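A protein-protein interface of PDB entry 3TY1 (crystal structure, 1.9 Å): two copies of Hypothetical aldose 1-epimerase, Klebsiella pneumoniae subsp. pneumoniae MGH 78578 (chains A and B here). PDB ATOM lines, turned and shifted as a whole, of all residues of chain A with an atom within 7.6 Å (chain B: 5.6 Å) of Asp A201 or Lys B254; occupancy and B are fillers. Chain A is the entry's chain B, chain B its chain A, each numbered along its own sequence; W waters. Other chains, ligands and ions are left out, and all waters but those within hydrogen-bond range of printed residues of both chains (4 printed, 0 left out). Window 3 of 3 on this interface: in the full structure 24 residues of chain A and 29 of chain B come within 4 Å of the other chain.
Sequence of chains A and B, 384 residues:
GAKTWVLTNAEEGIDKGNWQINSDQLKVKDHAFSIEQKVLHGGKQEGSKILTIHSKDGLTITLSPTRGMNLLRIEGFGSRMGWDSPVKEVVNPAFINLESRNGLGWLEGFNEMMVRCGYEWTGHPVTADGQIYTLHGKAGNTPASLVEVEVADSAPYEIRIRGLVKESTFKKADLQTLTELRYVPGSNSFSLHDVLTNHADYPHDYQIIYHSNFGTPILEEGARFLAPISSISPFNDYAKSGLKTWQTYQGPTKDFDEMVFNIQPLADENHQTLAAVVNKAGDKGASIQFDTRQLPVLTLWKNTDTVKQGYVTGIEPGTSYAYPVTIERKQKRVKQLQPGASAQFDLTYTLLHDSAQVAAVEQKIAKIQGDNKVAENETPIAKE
Of chain B, only Lys B254 (3.3 Å), Thr B306 (2.6 Å) and Lys B308 (3.4 Å) come within 4 Å of Asp A201. Lys B254 touches just these residues of chain A: Asp A201 and Tyr A202. Printed residues of chain A within 4 Å of Gln B309: Tyr A202. Printed residues of chain A within 4 Å of Asp B255: Tyr A202. Of the printed residues of chain A, Thr B306 touches Asp A201 (2.6 Å) and Tyr A202 (3.8 Å). Of the printed residues of chain A, Asp B305 touches Tyr A202 (2.6 Å). Asn A198 touches none of the printed residues of chain B. His A204 touches none of the printed residues of chain B. The nearest residue of chain B that does not touch Asp A201 is Gln B309 (4.3 Å). The nearest residue of chain A that does not touch Lys B254 is Pro A203 (5.1 Å).
Among the printed residues, pairs that only touch across the chains: His A199 with Lys B308, Asp A201 with Lys B308, Tyr A202 with Lys B254, Tyr A202 with Thr B306 and Tyr A202 with Gln B309.
No position is printed for both chains. Of the 9 pairs that touch across the chains among the printed residues, none has its exchanged pair printed and touching as well.
Hydrophobic or aromatic side chains of chain A that line the printed part of chain B: Tyr A202. Of the 11 printed residues of chain B, 6 touch a printed residue of chain A. Along chain B the printed residues that touch a printed residue of chain A span positions 254 to 309. Among the printed residues, no Asp or Glu carboxylate lies within 4 Å of a Lys or Arg side-chain nitrogen of the other chain.
Water W4 lies within hydrogen-bond range of OD2 of Asp A201 (2.6 Å), N of Lys B308 (3.2 Å) and N of Val B307 (3.4 Å). Water W1 bridges the side-chain carboxylate of Asp B305 (2.6 Å) and the side-chain hydroxyl of Tyr A202 (3.3 Å). Water W2 lies within hydrogen-bond range of OD1 of Asp A201 (2.7 Å) and NZ of Lys B308 (2.7 Å). Water W3 lies within hydrogen-bond range of the side-chain amide oxygen of Gln B309 (2.8 Å) and the backbone NH of Asp A201 (2.8 Å).
OH of Tyr A202 is in hydrogen-bond range of N of Asp B255 (2.7 Å). The side-chain hydroxyl of Thr B306 lies within hydrogen-bond range of the side-chain carboxylate of Asp A201, at 2.6 Å. NZ of Lys B254 lies within hydrogen-bond range of O of Asp A201. OD1 of Asp B305 is in hydrogen-bond range of OH of Tyr A202, 2.6 Å away.
N of His A199 lies within hydrogen-bond range of O of Asp A174, 2.8 Å away. The backbone NH of Thr B253 lies within hydrogen-bond range of the backbone carbonyl oxygen of Asp B305 (3.4 Å). ND2 of Asn A198 is in hydrogen-bond range of O of Tyr A202 (3.0 Å). The side-chain carboxylate of Asp B305 lies within hydrogen-bond range of the backbone NH of Phe B256 (3.1 Å). OG1 of Thr B306 sits at hydrogen-bond distance from N of Gln B309 (3.0 Å). N of Lys B308 lies close to OG1 of Thr B306, at 3.5 Å.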
ATOM      1  N   ASP A 174      17.397 -33.205 -29.053  1.00  0.00           N
ATOM      2  CA  ASP A 174      18.756 -33.014 -28.626  1.00  0.00           C
ATOM      3  C   ASP A 174      19.248 -34.344 -28.111  1.00  0.00           C
ATOM      4  O   ASP A 174      19.318 -34.568 -26.904  1.00  0.00           O
ATOM      5  CB  ASP A 174      18.901 -31.926 -27.582  1.00  0.00           C
ATOM      6  CG  ASP A 174      20.399 -31.497 -27.371  1.00  0.00           C
ATOM      7  OD1 ASP A 174      21.320 -32.057 -28.078  1.00  0.00           O
ATOM      8  OD2 ASP A 174      20.616 -30.656 -26.448  1.00  0.00           O
ATOM      9  N   ASN A 198      19.347 -38.275 -23.974  1.00  0.00           N
ATOM     10  CA  ASN A 198      18.370 -37.304 -24.355  1.00  0.00           C
ATOM     11  C   ASN A 198      18.612 -36.045 -23.507  1.00  0.00           C
ATOM     12  O   ASN A 198      18.269 -35.997 -22.327  1.00  0.00           O
ATOM     13  CB  ASN A 198      16.966 -37.852 -24.182  1.00  0.00           C
ATOM     14  CG  ASN A 198      15.923 -36.855 -24.556  1.00  0.00           C
ATOM     15  OD1 ASN A 198      16.235 -35.770 -25.080  1.00  0.00           O
ATOM     16  ND2 ASN A 198      14.673 -37.189 -24.277  1.00  0.00           N
ATOM     17  N   HIS A 199      19.267 -35.060 -24.098  1.00  0.00           N
ATOM     18  CA  HIS A 199      19.537 -33.778 -23.395  1.00  0.00           C
ATOM     19  C   HIS A 199      18.357 -32.777 -23.363  1.00  0.00           C
ATOM     20  O   HIS A 199      18.487 -31.710 -22.761  1.00  0.00           O
ATOM     21  CB  HIS A 199      20.716 -33.090 -24.066  1.00  0.00           C
ATOM     22  CG  HIS A 199      22.010 -33.799 -23.861  1.00  0.00           C
ATOM     23  ND1 HIS A 199      22.925 -33.396 -22.920  1.00  0.00           N
ATOM     24  CD2 HIS A 199      22.536 -34.906 -24.454  1.00  0.00           C
ATOM     25  CE1 HIS A 199      23.951 -34.232 -22.918  1.00  0.00           C
ATOM     26  NE2 HIS A 199      23.745 -35.154 -23.838  1.00  0.00           N
ATOM     27  N   ALA A 200      17.264 -33.082 -24.056  1.00  0.00           N
ATOM     28  CA  ALA A 200      16.050 -32.234 -24.065  1.00  0.00           C
ATOM     29  C   ALA A 200      15.210 -32.446 -22.811  1.00  0.00           C
ATOM     30  O   ALA A 200      15.422 -33.393 -22.051  1.00  0.00           O
ATOM     31  CB  ALA A 200      15.204 -32.564 -25.311  1.00  0.00           C
ATOM     32  N   ASP A 201      14.233 -31.561 -22.626  1.00  0.00           N
ATOM     33  CA  ASP A 201      13.255 -31.633 -21.564  1.00  0.00           C
ATOM     34  C   ASP A 201      11.994 -32.423 -21.911  1.00  0.00           C
ATOM     35  O   ASP A 201      11.088 -32.500 -21.071  1.00  0.00           O
ATOM     36  CB  ASP A 201      12.834 -30.219 -21.118  1.00  0.00           C
ATOM     37  CG  ASP A 201      13.826 -29.590 -20.151  1.00  0.00           C
ATOM     38  OD1 ASP A 201      14.520 -30.325 -19.420  1.00  0.00           O
ATOM     39  OD2 ASP A 201      13.920 -28.358 -20.138  1.00  0.00           O
ATOM     40  N   TYR A 202      11.947 -33.011 -23.107  1.00  0.00           N
ATOM     41  CA  TYR A 202      10.809 -33.806 -23.550  1.00  0.00           C
ATOM     42  C   TYR A 202      11.306 -35.188 -23.927  1.00  0.00           C
ATOM     43  O   TYR A 202      12.407 -35.307 -24.455  1.00  0.00           O
ATOM     44  CB  TYR A 202      10.131 -33.156 -24.771  1.00  0.00           C
ATOM     45  CG  TYR A 202       9.561 -31.807 -24.400  1.00  0.00           C
ATOM     46  CD1 TYR A 202       8.307 -31.709 -23.831  1.00  0.00           C
ATOM     47  CD2 TYR A 202      10.304 -30.630 -24.564  1.00  0.00           C
ATOM     48  CE1 TYR A 202       7.778 -30.469 -23.468  1.00  0.00           C
ATOM     49  CE2 TYR A 202       9.781 -29.377 -24.185  1.00  0.00           C
ATOM     50  CZ  TYR A 202       8.512 -29.313 -23.637  1.00  0.00           C
ATOM     51  OH  TYR A 202       7.957 -28.121 -23.216  1.00  0.00           O
ATOM     52  N   PRO A 203      10.479 -36.229 -23.699  1.00  0.00           N
ATOM     53  CA  PRO A 203      10.864 -37.567 -24.202  1.00  0.00           C
ATOM     54  C   PRO A 203      11.029 -37.514 -25.698  1.00  0.00           C
ATOM     55  O   PRO A 203      10.372 -36.701 -26.353  1.00  0.00           O
ATOM     56  CB  PRO A 203       9.670 -38.472 -23.813  1.00  0.00           C
ATOM     57  CG  PRO A 203       8.662 -37.655 -23.131  1.00  0.00           C
ATOM     58  CD  PRO A 203       9.127 -36.215 -23.082  1.00  0.00           C
ATOM     59  N   HIS A 204      11.913 -38.333 -26.252  1.00  0.00           N
ATOM     60  CA  HIS A 204      12.092 -38.381 -27.688  1.00  0.00           C
ATOM     61  C   HIS A 204      12.315 -39.805 -28.161  1.00  0.00           C
ATOM     62  O   HIS A 204      12.989 -40.590 -27.467  1.00  0.00           O
ATOM     63  CB  HIS A 204      13.318 -37.547 -28.132  1.00  0.00           C
ATOM     64  CG  HIS A 204      13.280 -37.167 -29.579  1.00  0.00           C
ATOM     65  ND1 HIS A 204      13.584 -38.051 -30.588  1.00  0.00           N
ATOM     66  CD2 HIS A 204      12.888 -36.018 -30.189  1.00  0.00           C
ATOM     67  CE1 HIS A 204      13.386 -37.473 -31.761  1.00  0.00           C
ATOM     68  NE2 HIS A 204      12.954 -36.241 -31.550  1.00  0.00           N
ATOM     69  N   GLN A 338      13.560 -40.910 -21.884  1.00  0.00           N
ATOM     70  CA  GLN A 338      13.030 -39.857 -21.035  1.00  0.00           C
ATOM     71  C   GLN A 338      13.961 -38.646 -21.052  1.00  0.00           C
ATOM     72  O   GLN A 338      15.146 -38.787 -21.292  1.00  0.00           O
ATOM     73  CB  GLN A 338      12.835 -40.333 -19.575  1.00  0.00           C
ATOM     74  CG  GLN A 338      11.789 -41.409 -19.440  1.00  0.00           C
ATOM     75  CD  GLN A 338      10.439 -40.939 -19.925  1.00  0.00           C
ATOM     76  OE1 GLN A 338       9.898 -41.470 -20.901  1.00  0.00           O
ATOM     77  NE2 GLN A 338       9.921 -39.916 -19.286  1.00  0.00           N
ATOM     78  N   PRO A 339      13.434 -37.477 -20.717  1.00  0.00           N
ATOM     79  CA  PRO A 339      14.296 -36.310 -20.687  1.00  0.00           C
ATOM     80  C   PRO A 339      15.446 -36.470 -19.679  1.00  0.00           C
ATOM     81  O   PRO A 339      15.230 -36.882 -18.551  1.00  0.00           O
ATOM     82  CB  PRO A 339      13.342 -35.182 -20.288  1.00  0.00           C
ATOM     83  CG  PRO A 339      12.059 -35.748 -20.026  1.00  0.00           C
ATOM     84  CD  PRO A 339      12.019 -37.118 -20.564  1.00  0.00           C
ATOM     85  N   GLY A 340      16.667 -36.230 -20.129  1.00  0.00           N
ATOM     86  CA  GLY A 340      17.860 -36.374 -19.296  1.00  0.00           C
ATOM     87  C   GLY A 340      18.349 -37.818 -19.140  1.00  0.00           C
ATOM     88  O   GLY A 340      19.412 -38.025 -18.544  1.00  0.00           O
ATOM     89  N   PRO B 252       9.546 -19.855 -17.774  1.00  0.00           N
ATOM     90  CA  PRO B 252       9.729 -21.044 -18.629  1.00  0.00           C
ATOM     91  C   PRO B 252       8.612 -22.055 -18.413  1.00  0.00           C
ATOM     92  O   PRO B 252       8.398 -22.480 -17.289  1.00  0.00           O
ATOM     93  CB  PRO B 252      11.077 -21.598 -18.173  1.00  0.00           C
ATOM     94  CG  PRO B 252      11.798 -20.405 -17.582  1.00  0.00           C
ATOM     95  CD  PRO B 252      10.743 -19.573 -16.952  1.00  0.00           C
ATOM     96  N   THR B 253       7.852 -22.352 -19.464  1.00  0.00           N
ATOM     97  CA  THR B 253       6.627 -23.130 -19.340  1.00  0.00           C
ATOM     98  C   THR B 253       6.649 -24.383 -20.210  1.00  0.00           C
ATOM     99  O   THR B 253       6.749 -24.305 -21.417  1.00  0.00           O
ATOM    100  CB  THR B 253       5.416 -22.254 -19.705  1.00  0.00           C
ATOM    101  OG1 THR B 253       5.492 -21.026 -18.976  1.00  0.00           O
ATOM    102  CG2 THR B 253       4.094 -22.963 -19.409  1.00  0.00           C
ATOM    103  N   LYS B 254       6.555 -25.549 -19.582  1.00  0.00           N
ATOM    104  CA  LYS B 254       6.558 -26.815 -20.330  1.00  0.00           C
ATOM    105  C   LYS B 254       5.311 -26.853 -21.228  1.00  0.00           C
ATOM    106  O   LYS B 254       4.257 -26.404 -20.809  1.00  0.00           O
ATOM    107  CB  LYS B 254       6.542 -27.986 -19.332  1.00  0.00           C
ATOM    108  CG  LYS B 254       6.521 -29.385 -19.937  1.00  0.00           C
ATOM    109  CD  LYS B 254       6.673 -30.447 -18.828  1.00  0.00           C
ATOM    110  CE  LYS B 254       6.661 -31.866 -19.393  1.00  0.00           C
ATOM    111  NZ  LYS B 254       7.876 -32.136 -20.234  1.00  0.00           N
ATOM    112  N   ASP B 255       5.441 -27.381 -22.441  1.00  0.00           N
ATOM    113  CA  ASP B 255       4.336 -27.539 -23.410  1.00  0.00           C
ATOM    114  C   ASP B 255       3.780 -26.258 -23.998  1.00  0.00           C
ATOM    115  O   ASP B 255       2.706 -26.269 -24.618  1.00  0.00           O
ATOM    116  CB  ASP B 255       3.168 -28.371 -22.826  1.00  0.00           C
ATOM    117  CG  ASP B 255       3.611 -29.767 -22.396  1.00  0.00           C
ATOM    118  OD1 ASP B 255       4.383 -30.409 -23.142  1.00  0.00           O
ATOM    119  OD2 ASP B 255       3.176 -30.209 -21.321  1.00  0.00           O
ATOM    120  N   PHE B 256       4.513 -25.166 -23.858  1.00  0.00           N
ATOM    121  CA  PHE B 256       4.027 -23.887 -24.340  1.00  0.00           C
ATOM    122  C   PHE B 256       4.265 -23.768 -25.838  1.00  0.00           C
ATOM    123  O   PHE B 256       3.420 -23.248 -26.570  1.00  0.00           O
ATOM    124  CB  PHE B 256       4.775 -22.778 -23.620  1.00  0.00           C
ATOM    125  CG  PHE B 256       4.289 -21.403 -23.970  1.00  0.00           C
ATOM    126  CD1 PHE B 256       3.202 -20.859 -23.310  1.00  0.00           C
ATOM    127  CD2 PHE B 256       4.912 -20.670 -24.966  1.00  0.00           C
ATOM    128  CE1 PHE B 256       2.733 -19.601 -23.632  1.00  0.00           C
ATOM    129  CE2 PHE B 256       4.457 -19.408 -25.296  1.00  0.00           C
ATOM    130  CZ  PHE B 256       3.371 -18.862 -24.614  1.00  0.00           C
ATOM    131  N   THR B 304       8.278 -18.942 -24.789  1.00  0.00           N
ATOM    132  CA  THR B 304       8.509 -19.086 -23.350  1.00  0.00           C
ATOM    133  C   THR B 304       8.329 -20.537 -22.896  1.00  0.00           C
ATOM    134  O   THR B 304       7.603 -20.828 -21.945  1.00  0.00           O
ATOM    135  CB  THR B 304       7.663 -18.096 -22.553  1.00  0.00           C
ATOM    136  OG1 THR B 304       6.297 -18.223 -22.970  1.00  0.00           O
ATOM    137  CG2 THR B 304       8.180 -16.677 -22.821  1.00  0.00           C
ATOM    138  N   ASP B 305       9.060 -21.442 -23.560  1.00  0.00           N
ATOM    139  CA  ASP B 305       9.036 -22.861 -23.235  1.00  0.00           C
ATOM    140  C   ASP B 305      10.136 -23.105 -22.155  1.00  0.00           C
ATOM    141  O   ASP B 305      10.565 -22.161 -21.463  1.00  0.00           O
ATOM    142  CB  ASP B 305       9.211 -23.716 -24.528  1.00  0.00           C
ATOM    143  CG  ASP B 305       8.599 -25.130 -24.410  1.00  0.00           C
ATOM    144  OD1 ASP B 305       9.234 -25.985 -23.805  1.00  0.00           O
ATOM    145  OD2 ASP B 305       7.476 -25.385 -24.895  1.00  0.00           O
ATOM    146  N   THR B 306      10.610 -24.342 -22.002  1.00  0.00           N
ATOM    147  CA  THR B 306      11.575 -24.645 -20.959  1.00  0.00           C
ATOM    148  C   THR B 306      12.923 -24.039 -21.370  1.00  0.00           C
ATOM    149  O   THR B 306      13.184 -23.731 -22.565  1.00  0.00           O
ATOM    150  CB  THR B 306      11.753 -26.181 -20.704  1.00  0.00           C
ATOM    151  OG1 THR B 306      12.585 -26.733 -21.733  1.00  0.00           O
ATOM    152  CG2 THR B 306      10.423 -26.943 -20.624  1.00  0.00           C
ATOM    153  N   VAL B 307      13.813 -23.870 -20.392  1.00  0.00           N
ATOM    154  CA  VAL B 307      15.110 -23.287 -20.676  1.00  0.00           C
ATOM    155  C   VAL B 307      15.908 -24.157 -21.660  1.00  0.00           C
ATOM    156  O   VAL B 307      16.526 -23.647 -22.585  1.00  0.00           O
ATOM    157  CB  VAL B 307      15.916 -22.930 -19.404  1.00  0.00           C
ATOM    158  CG1 VAL B 307      17.291 -22.407 -19.799  1.00  0.00           C
ATOM    159  CG2 VAL B 307      15.176 -21.823 -18.526  1.00  0.00           C
ATOM    160  N   LYS B 308      15.818 -25.472 -21.534  1.00  0.00           N
ATOM    161  CA  LYS B 308      16.523 -26.347 -22.497  1.00  0.00           C
ATOM    162  C   LYS B 308      15.865 -26.346 -23.871  1.00  0.00           C
ATOM    163  O   LYS B 308      16.570 -26.350 -24.899  1.00  0.00           O
ATOM    164  CB  LYS B 308      16.689 -27.780 -21.957  1.00  0.00           C
ATOM    165  CG  LYS B 308      17.681 -27.850 -20.798  1.00  0.00           C
ATOM    166  CD  LYS B 308      17.955 -29.272 -20.291  1.00  0.00           C
ATOM    167  CE  LYS B 308      18.845 -29.204 -19.016  1.00  0.00           C
ATOM    168  NZ  LYS B 308      18.796 -30.412 -18.129  1.00  0.00           N
ATOM    169  N   GLN B 309      14.539 -26.331 -23.910  1.00  0.00           N
ATOM    170  CA  GLN B 309      13.834 -26.309 -25.195  1.00  0.00           C
ATOM    171  C   GLN B 309      14.043 -24.999 -25.933  1.00  0.00           C
ATOM    172  O   GLN B 309      14.159 -24.991 -27.139  1.00  0.00           O
ATOM    173  CB  GLN B 309      12.353 -26.551 -25.026  1.00  0.00           C
ATOM    174  CG  GLN B 309      11.548 -26.651 -26.327  1.00  0.00           C
ATOM    175  CD  GLN B 309      11.704 -28.008 -27.057  1.00  0.00           C
ATOM    176  OE1 GLN B 309      12.500 -28.857 -26.661  1.00  0.00           O
ATOM    177  NE2 GLN B 309      10.942 -28.184 -28.131  1.00  0.00           N
HETATM  178  O   HOH W   1       7.053 -27.487 -26.364  1.00  0.00           O
HETATM  179  O   HOH W   2      16.230 -29.965 -17.398  1.00  0.00           O
HETATM  180  O   HOH W   3      14.176 -29.512 -24.572  1.00  0.00           O
HETATM  181  O   HOH W   4      14.894 -26.540 -18.631  1.00  0.00           O
